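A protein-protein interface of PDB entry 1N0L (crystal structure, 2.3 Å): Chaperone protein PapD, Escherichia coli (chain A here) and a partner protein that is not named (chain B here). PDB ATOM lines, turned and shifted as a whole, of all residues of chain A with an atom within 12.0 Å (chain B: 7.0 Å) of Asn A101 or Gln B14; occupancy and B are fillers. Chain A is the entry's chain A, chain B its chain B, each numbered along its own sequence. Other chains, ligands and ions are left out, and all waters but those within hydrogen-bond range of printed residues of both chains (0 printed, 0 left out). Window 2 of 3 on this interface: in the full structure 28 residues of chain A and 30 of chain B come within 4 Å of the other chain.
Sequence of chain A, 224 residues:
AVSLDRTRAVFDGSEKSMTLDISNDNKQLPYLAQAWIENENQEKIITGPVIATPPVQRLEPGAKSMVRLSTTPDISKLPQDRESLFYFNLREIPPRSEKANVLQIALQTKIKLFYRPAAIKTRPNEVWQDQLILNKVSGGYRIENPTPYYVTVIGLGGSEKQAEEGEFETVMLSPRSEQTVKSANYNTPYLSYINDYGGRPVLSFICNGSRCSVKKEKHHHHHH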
ATOM      1  N   ARG A  96     -20.661  -5.710 -22.296  1.00  0.00           N
ATOM      2  CA  ARG A  96     -20.772  -7.111 -21.926  1.00  0.00           C
ATOM      3  C   ARG A  96     -22.184  -7.418 -21.453  1.00  0.00           C
ATOM      4  O   ARG A  96     -22.668  -6.827 -20.488  1.00  0.00           O
ATOM      5  CB  ARG A  96     -19.758  -7.449 -20.834  1.00  0.00           C
ATOM      6  CG  ARG A  96     -19.725  -6.472 -19.673  1.00  0.00           C
ATOM      7  CD  ARG A  96     -18.661  -6.861 -18.649  1.00  0.00           C
ATOM      8  NE  ARG A  96     -19.088  -7.914 -17.724  1.00  0.00           N
ATOM      9  CZ  ARG A  96     -19.292  -9.190 -18.049  1.00  0.00           C
ATOM     10  NH1 ARG A  96     -19.114  -9.612 -19.293  1.00  0.00           N
ATOM     11  NH2 ARG A  96     -19.667 -10.055 -17.114  1.00  0.00           N
ATOM     12  N   SER A  97     -22.850  -8.331 -22.150  1.00  0.00           N
ATOM     13  CA  SER A  97     -24.210  -8.707 -21.788  1.00  0.00           C
ATOM     14  C   SER A  97     -24.237  -9.297 -20.384  1.00  0.00           C
ATOM     15  O   SER A  97     -23.430 -10.164 -20.043  1.00  0.00           O
ATOM     16  CB  SER A  97     -24.770  -9.726 -22.782  1.00  0.00           C
ATOM     17  OG  SER A  97     -26.071 -10.138 -22.397  1.00  0.00           O
ATOM     18  N   GLU A  98     -25.170  -8.816 -19.570  1.00  0.00           N
ATOM     19  CA  GLU A  98     -25.307  -9.297 -18.203  1.00  0.00           C
ATOM     20  C   GLU A  98     -25.899 -10.702 -18.202  1.00  0.00           C
ATOM     21  O   GLU A  98     -25.919 -11.373 -17.171  1.00  0.00           O
ATOM     22  CB  GLU A  98     -26.213  -8.358 -17.404  1.00  0.00           C
ATOM     23  CG  GLU A  98     -25.718  -6.924 -17.329  1.00  0.00           C
ATOM     24  CD  GLU A  98     -26.653  -6.029 -16.539  1.00  0.00           C
ATOM     25  OE1 GLU A  98     -27.833  -5.903 -16.930  1.00  0.00           O
ATOM     26  OE2 GLU A  98     -26.207  -5.449 -15.526  1.00  0.00           O
ATOM     27  N   LYS A  99     -26.371 -11.140 -19.367  1.00  0.00           N
ATOM     28  CA  LYS A  99     -26.979 -12.459 -19.512  1.00  0.00           C
ATOM     29  C   LYS A  99     -25.958 -13.597 -19.491  1.00  0.00           C
ATOM     30  O   LYS A  99     -24.750 -13.365 -19.544  1.00  0.00           O
ATOM     31  CB  LYS A  99     -27.795 -12.503 -20.805  1.00  0.00           C
ATOM     32  CG  LYS A  99     -28.841 -11.403 -20.876  1.00  0.00           C
ATOM     33  CD  LYS A  99     -29.697 -11.485 -22.128  1.00  0.00           C
ATOM     34  CE  LYS A  99     -30.687 -10.327 -22.172  1.00  0.00           C
ATOM     35  NZ  LYS A  99     -31.567 -10.371 -23.371  1.00  0.00           N
ATOM     36  N   ALA A 100     -26.454 -14.829 -19.405  1.00  0.00           N
ATOM     37  CA  ALA A 100     -25.589 -16.004 -19.368  1.00  0.00           C
ATOM     38  C   ALA A 100     -25.849 -16.930 -20.553  1.00  0.00           C
ATOM     39  O   ALA A 100     -26.975 -17.023 -21.044  1.00  0.00           O
ATOM     40  CB  ALA A 100     -25.796 -16.759 -18.060  1.00  0.00           C
ATOM     41  N   ASN A 101     -24.801 -17.621 -20.994  1.00  0.00           N
ATOM     42  CA  ASN A 101     -24.886 -18.536 -22.133  1.00  0.00           C
ATOM     43  C   ASN A 101     -25.332 -17.737 -23.355  1.00  0.00           C
ATOM     44  O   ASN A 101     -26.341 -18.058 -23.992  1.00  0.00           O
ATOM     45  CB  ASN A 101     -25.892 -19.660 -21.860  1.00  0.00           C
ATOM     46  CG  ASN A 101     -25.790 -20.207 -20.447  1.00  0.00           C
ATOM     47  OD1 ASN A 101     -24.700 -20.497 -19.952  1.00  0.00           O
ATOM     48  ND2 ASN A 101     -26.937 -20.359 -19.791  1.00  0.00           N
ATOM     49  N   VAL A 102     -24.564 -16.700 -23.676  1.00  0.00           N
ATOM     50  CA  VAL A 102     -24.874 -15.824 -24.798  1.00  0.00           C
ATOM     51  C   VAL A 102     -23.713 -15.606 -25.767  1.00  0.00           C
ATOM     52  O   VAL A 102     -22.555 -15.472 -25.353  1.00  0.00           O
ATOM     53  CB  VAL A 102     -25.319 -14.441 -24.290  1.00  0.00           C
ATOM     54  CG1 VAL A 102     -26.553 -14.582 -23.408  1.00  0.00           C
ATOM     55  CG2 VAL A 102     -24.178 -13.785 -23.511  1.00  0.00           C
ATOM     56  N   LEU A 103     -24.039 -15.570 -27.058  1.00  0.00           N
ATOM     57  CA  LEU A 103     -23.049 -15.323 -28.100  1.00  0.00           C
ATOM     58  C   LEU A 103     -23.258 -13.912 -28.636  1.00  0.00           C
ATOM     59  O   LEU A 103     -24.284 -13.614 -29.255  1.00  0.00           O
ATOM     60  CB  LEU A 103     -23.184 -16.313 -29.254  1.00  0.00           C
ATOM     61  CG  LEU A 103     -22.270 -15.955 -30.433  1.00  0.00           C
ATOM     62  CD1 LEU A 103     -20.819 -15.959 -29.971  1.00  0.00           C
ATOM     63  CD2 LEU A 103     -22.476 -16.932 -31.575  1.00  0.00           C
ATOM     64  N   GLN A 104     -22.280 -13.050 -28.388  1.00  0.00           N
ATOM     65  CA  GLN A 104     -22.337 -11.667 -28.836  1.00  0.00           C
ATOM     66  C   GLN A 104     -21.849 -11.512 -30.277  1.00  0.00           C
ATOM     67  O   GLN A 104     -20.835 -12.098 -30.666  1.00  0.00           O
ATOM     68  CB  GLN A 104     -21.475 -10.795 -27.924  1.00  0.00           C
ATOM     69  CG  GLN A 104     -21.486  -9.332 -28.287  1.00  0.00           C
ATOM     70  CD  GLN A 104     -22.748  -8.624 -27.837  1.00  0.00           C
ATOM     71  OE1 GLN A 104     -22.920  -8.333 -26.652  1.00  0.00           O
ATOM     72  NE2 GLN A 104     -23.645  -8.349 -28.783  1.00  0.00           N
ATOM     73  N   ILE A 105     -22.586 -10.736 -31.066  1.00  0.00           N
ATOM     74  CA  ILE A 105     -22.208 -10.467 -32.450  1.00  0.00           C
ATOM     75  C   ILE A 105     -21.667  -9.043 -32.504  1.00  0.00           C
ATOM     76  O   ILE A 105     -22.367  -8.097 -32.153  1.00  0.00           O
ATOM     77  CB  ILE A 105     -23.406 -10.557 -33.414  1.00  0.00           C
ATOM     78  CG1 ILE A 105     -23.830 -12.013 -33.601  1.00  0.00           C
ATOM     79  CG2 ILE A 105     -23.030  -9.949 -34.754  1.00  0.00           C
ATOM     80  CD1 ILE A 105     -22.746 -12.899 -34.179  1.00  0.00           C
ATOM     81  N   VAL B  11     -27.573 -14.138 -29.254  1.00  0.00           N
ATOM     82  CA  VAL B  11     -28.417 -15.328 -29.221  1.00  0.00           C
ATOM     83  C   VAL B  11     -28.347 -15.942 -27.823  1.00  0.00           C
ATOM     84  O   VAL B  11     -27.289 -15.917 -27.186  1.00  0.00           O
ATOM     85  CB  VAL B  11     -27.957 -16.367 -30.268  1.00  0.00           C
ATOM     86  CG1 VAL B  11     -26.550 -16.835 -29.950  1.00  0.00           C
ATOM     87  CG2 VAL B  11     -28.929 -17.536 -30.305  1.00  0.00           C
ATOM     88  N   ASP B  12     -29.467 -16.496 -27.355  1.00  0.00           N
ATOM     89  CA  ASP B  12     -29.541 -17.080 -26.014  1.00  0.00           C
ATOM     90  C   ASP B  12     -29.666 -18.588 -25.868  1.00  0.00           C
ATOM     91  O   ASP B  12     -30.088 -19.301 -26.779  1.00  0.00           O
ATOM     92  CB  ASP B  12     -30.692 -16.448 -25.229  1.00  0.00           C
ATOM     93  CG  ASP B  12     -30.311 -15.136 -24.592  1.00  0.00           C
ATOM     94  OD1 ASP B  12     -29.331 -15.117 -23.817  1.00  0.00           O
ATOM     95  OD2 ASP B  12     -30.992 -14.127 -24.865  1.00  0.00           O
ATOM     96  N   TRP B  13     -29.302 -19.045 -24.673  1.00  0.00           N
ATOM     97  CA  TRP B  13     -29.363 -20.445 -24.277  1.00  0.00           C
ATOM     98  C   TRP B  13     -29.641 -20.486 -22.778  1.00  0.00           C
ATOM     99  O   TRP B  13     -29.006 -19.766 -22.002  1.00  0.00           O
ATOM    100  CB  TRP B  13     -28.047 -21.152 -24.587  1.00  0.00           C
ATOM    101  CG  TRP B  13     -27.928 -21.551 -26.016  1.00  0.00           C
ATOM    102  CD1 TRP B  13     -28.669 -22.493 -26.668  1.00  0.00           C
ATOM    103  CD2 TRP B  13     -27.021 -21.014 -26.978  1.00  0.00           C
ATOM    104  NE1 TRP B  13     -28.278 -22.579 -27.981  1.00  0.00           N
ATOM    105  CE2 TRP B  13     -27.266 -21.682 -28.199  1.00  0.00           C
ATOM    106  CE3 TRP B  13     -26.023 -20.032 -26.929  1.00  0.00           C
ATOM    107  CZ2 TRP B  13     -26.547 -21.397 -29.366  1.00  0.00           C
ATOM    108  CZ3 TRP B  13     -25.307 -19.749 -28.090  1.00  0.00           C
ATOM    109  CH2 TRP B  13     -25.574 -20.432 -29.293  1.00  0.00           C
ATOM    110  N   GLN B  14     -30.597 -21.319 -22.376  1.00  0.00           N
ATOM    111  CA  GLN B  14     -30.967 -21.432 -20.971  1.00  0.00           C
ATOM    112  C   GLN B  14     -30.123 -22.462 -20.231  1.00  0.00           C
ATOM    113  O   GLN B  14     -29.725 -22.244 -19.086  1.00  0.00           O
ATOM    114  CB  GLN B  14     -32.450 -21.787 -20.849  1.00  0.00           C
ATOM    115  CG  GLN B  14     -33.368 -20.868 -21.650  1.00  0.00           C
ATOM    116  CD  GLN B  14     -33.011 -19.392 -21.501  1.00  0.00           C
ATOM    117  OE1 GLN B  14     -32.893 -18.875 -20.387  1.00  0.00           O
ATOM    118  NE2 GLN B  14     -32.843 -18.705 -22.630  1.00  0.00           N
ATOM    119  N   ASP B  15     -29.849 -23.581 -20.894  1.00  0.00           N
ATOM    120  CA  ASP B  15     -29.052 -24.654 -20.309  1.00  0.00           C
ATOM    121  C   ASP B  15     -29.188 -25.900 -21.175  1.00  0.00           C
ATOM    122  O   ASP B  15     -30.289 -26.229 -21.625  1.00  0.00           O
ATOM    123  CB  ASP B  15     -29.540 -24.977 -18.896  1.00  0.00           C
ATOM    124  CG  ASP B  15     -30.970 -25.485 -18.880  1.00  0.00           C
ATOM    125  OD1 ASP B  15     -31.889 -24.702 -19.208  1.00  0.00           O
ATOM    126  OD2 ASP B  15     -31.172 -26.672 -18.547  1.00  0.00           O
ATOM    127  N   VAL B  16     -28.075 -26.590 -21.408  1.00  0.00           N
ATOM    128  CA  VAL B  16     -28.104 -27.801 -22.220  1.00  0.00           C
ATOM    129  C   VAL B  16     -27.036 -28.803 -21.773  1.00  0.00           C
ATOM    130  O   VAL B  16     -26.409 -29.469 -22.598  1.00  0.00           O
ATOM    131  CB  VAL B  16     -27.894 -27.478 -23.723  1.00  0.00           C
ATOM    132  CG1 VAL B  16     -28.405 -28.626 -24.567  1.00  0.00           C
ATOM    133  CG2 VAL B  16     -28.610 -26.194 -24.100  1.00  0.00           C
ATOM    134  N   LYS B  29     -30.678 -23.416 -33.674  1.00  0.00           N
ATOM    135  CA  LYS B  29     -31.226 -22.156 -33.195  1.00  0.00           C
ATOM    136  C   LYS B  29     -31.323 -21.106 -34.286  1.00  0.00           C
ATOM    137  O   LYS B  29     -30.469 -21.016 -35.169  1.00  0.00           O
ATOM    138  CB  LYS B  29     -30.394 -21.622 -32.028  1.00  0.00           C
ATOM    139  CG  LYS B  29     -30.962 -20.361 -31.403  1.00  0.00           C
ATOM    140  CD  LYS B  29     -30.803 -20.379 -29.890  1.00  0.00           C
ATOM    141  CE  LYS B  29     -31.579 -21.537 -29.269  1.00  0.00           C
ATOM    142  NZ  LYS B  29     -31.487 -21.557 -27.782  1.00  0.00           N
ATOM    143  N   LEU B  71     -16.055 -24.408 -25.092  1.00  0.00           N
ATOM    144  CA  LEU B  71     -17.321 -24.731 -25.729  1.00  0.00           C
ATOM    145  C   LEU B  71     -17.213 -24.447 -27.218  1.00  0.00           C
ATOM    146  O   LEU B  71     -16.356 -23.677 -27.652  1.00  0.00           O
ATOM    147  CB  LEU B  71     -18.452 -23.903 -25.121  1.00  0.00           C
ATOM    148  CG  LEU B  71     -19.854 -24.453 -25.388  1.00  0.00           C
ATOM    149  CD1 LEU B  71     -20.010 -25.796 -24.686  1.00  0.00           C
ATOM    150  CD2 LEU B  71     -20.901 -23.478 -24.879  1.00  0.00           C
ATOM    151  N   PRO B 126     -21.854 -20.128 -17.315  1.00  0.00           N
ATOM    152  CA  PRO B 126     -21.937 -18.705 -17.657  1.00  0.00           C
ATOM    153  C   PRO B 126     -20.862 -18.272 -18.654  1.00  0.00           C
ATOM    154  O   PRO B 126     -19.810 -17.756 -18.263  1.00  0.00           O
ATOM    155  CB  PRO B 126     -21.782 -18.023 -16.301  1.00  0.00           C
ATOM    156  CG  PRO B 126     -22.461 -18.985 -15.386  1.00  0.00           C
ATOM    157  CD  PRO B 126     -21.916 -20.316 -15.855  1.00  0.00           C
ATOM    158  N   PHE B 127     -21.135 -18.483 -19.940  1.00  0.00           N
ATOM    159  CA  PHE B 127     -20.197 -18.121 -20.997  1.00  0.00           C
ATOM    160  C   PHE B 127     -20.726 -16.975 -21.853  1.00  0.00           C
ATOM    161  O   PHE B 127     -21.925 -16.887 -22.114  1.00  0.00           O
ATOM    162  CB  PHE B 127     -19.901 -19.343 -21.878  1.00  0.00           C
ATOM    163  CG  PHE B 127     -21.084 -19.830 -22.679  1.00  0.00           C
ATOM    164  CD1 PHE B 127     -21.471 -19.182 -23.848  1.00  0.00           C
ATOM    165  CD2 PHE B 127     -21.806 -20.944 -22.268  1.00  0.00           C
ATOM    166  CE1 PHE B 127     -22.559 -19.638 -24.594  1.00  0.00           C
ATOM    167  CE2 PHE B 127     -22.896 -21.406 -23.010  1.00  0.00           C
ATOM    168  CZ  PHE B 127     -23.272 -20.752 -24.173  1.00  0.00           C
ATOM    169  N   SER B 128     -19.828 -16.092 -22.279  1.00  0.00           N
ATOM    170  CA  SER B 128     -20.209 -14.957 -23.114  1.00  0.00           C
ATOM    171  C   SER B 128     -19.247 -14.846 -24.293  1.00  0.00           C
ATOM    172  O   SER B 128     -18.368 -13.983 -24.320  1.00  0.00           O
ATOM    173  CB  SER B 128     -20.192 -13.660 -22.295  1.00  0.00           C
ATOM    174  OG  SER B 128     -18.897 -13.385 -21.791  1.00  0.00           O
ATOM    175  N   ALA B 129     -19.425 -15.735 -25.265  1.00  0.00           N
ATOM    176  CA  ALA B 129     -18.583 -15.767 -26.453  1.00  0.00           C
ATOM    177  C   ALA B 129     -18.905 -14.625 -27.406  1.00  0.00           C
ATOM    178  O   ALA B 129     -20.023 -14.109 -27.422  1.00  0.00           O
ATOM    179  CB  ALA B 129     -18.757 -17.097 -27.170  1.00  0.00           C
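The backbone carbonyl oxygen of Phe B127 lies within hydrogen-bond range of the backbone NH of Val A102 (3.1 Å).
The backbone carbonyl oxygen of Trp B13 is in hydrogen-bond range of the side-chain amide nitrogen of Asn A101 (3.1 Å).
N of Asn A101 is in hydrogen-bond range of O of Phe B127, 3.2 Å away.
The side-chain amide nitrogen (ND2) of Asn A101 sits at hydrogen-bond distance from the backbone carbonyl oxygen (O) of Gln B14 (3.4 Å).
The backbone carbonyl oxygen (O) of Val A102 lies within hydrogen-bond range of the backbone NH (N) of Ala B129 (3.1 Å).
The backbone NH (N) of Leu A103 sits at hydrogen-bond distance from the backbone carbonyl oxygen (O) of Val B11 (3.3 Å).
The backbone carbonyl oxygen (O) of Ala B129 sits at hydrogen-bond distance from the backbone NH (N) of Gln A104, 2.7 Å away.
The side-chain amino group of Lys B29 is in hydrogen-bond range of the backbone carbonyl oxygen of Asp B12 (2.8 Å).
Among the printed residues, merely in contact across the chains: Val A102 with Asp B12 (2.9 Å), Leu A103 with Ala B129 (3.2 Å), Val A102 with Ser B128 (3.3 Å), Val A102 with Val B11 (3.4 Å), Ala A100 with Trp B13 (3.5 Å), Asn A101 with Asp B12 (3.9 Å), Asn A101 with Pro B126 (3.9 Å) and Asn A101 with Val B11 (3.96 Å).
Printed residues of chain B within 4 Å of Ala A100: Trp B13 (3.5 Å).
Asn A101 touches six residues of chain B.
Of the printed residues of chain B, Val A102 touches Val B11, Asp B12, Phe B127, Ser B128 and Ala B129.
Of the printed residues of chain B, Gln A104 touches Ala B129.
Val B11 touches three residues of chain A.
Of the printed residues of chain A, Asp B12 touches Asn A101 and Val A102.
Of chain A, only Asn A101 and Val A102 come within 4 Å of Phe B127.
Of the printed residues of chain A, Ser B128 touches Val A102 (3.3 Å).
Of the 10 printed residues of chain A, 5 touch a printed residue of chain B.
Printed residues of chain A that touch a printed residue of chain B: Ala A100, Asn A101, Val A102, Leu A103 and Gln A104.
Among the printed residues, 15 pairs touch across the chains.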
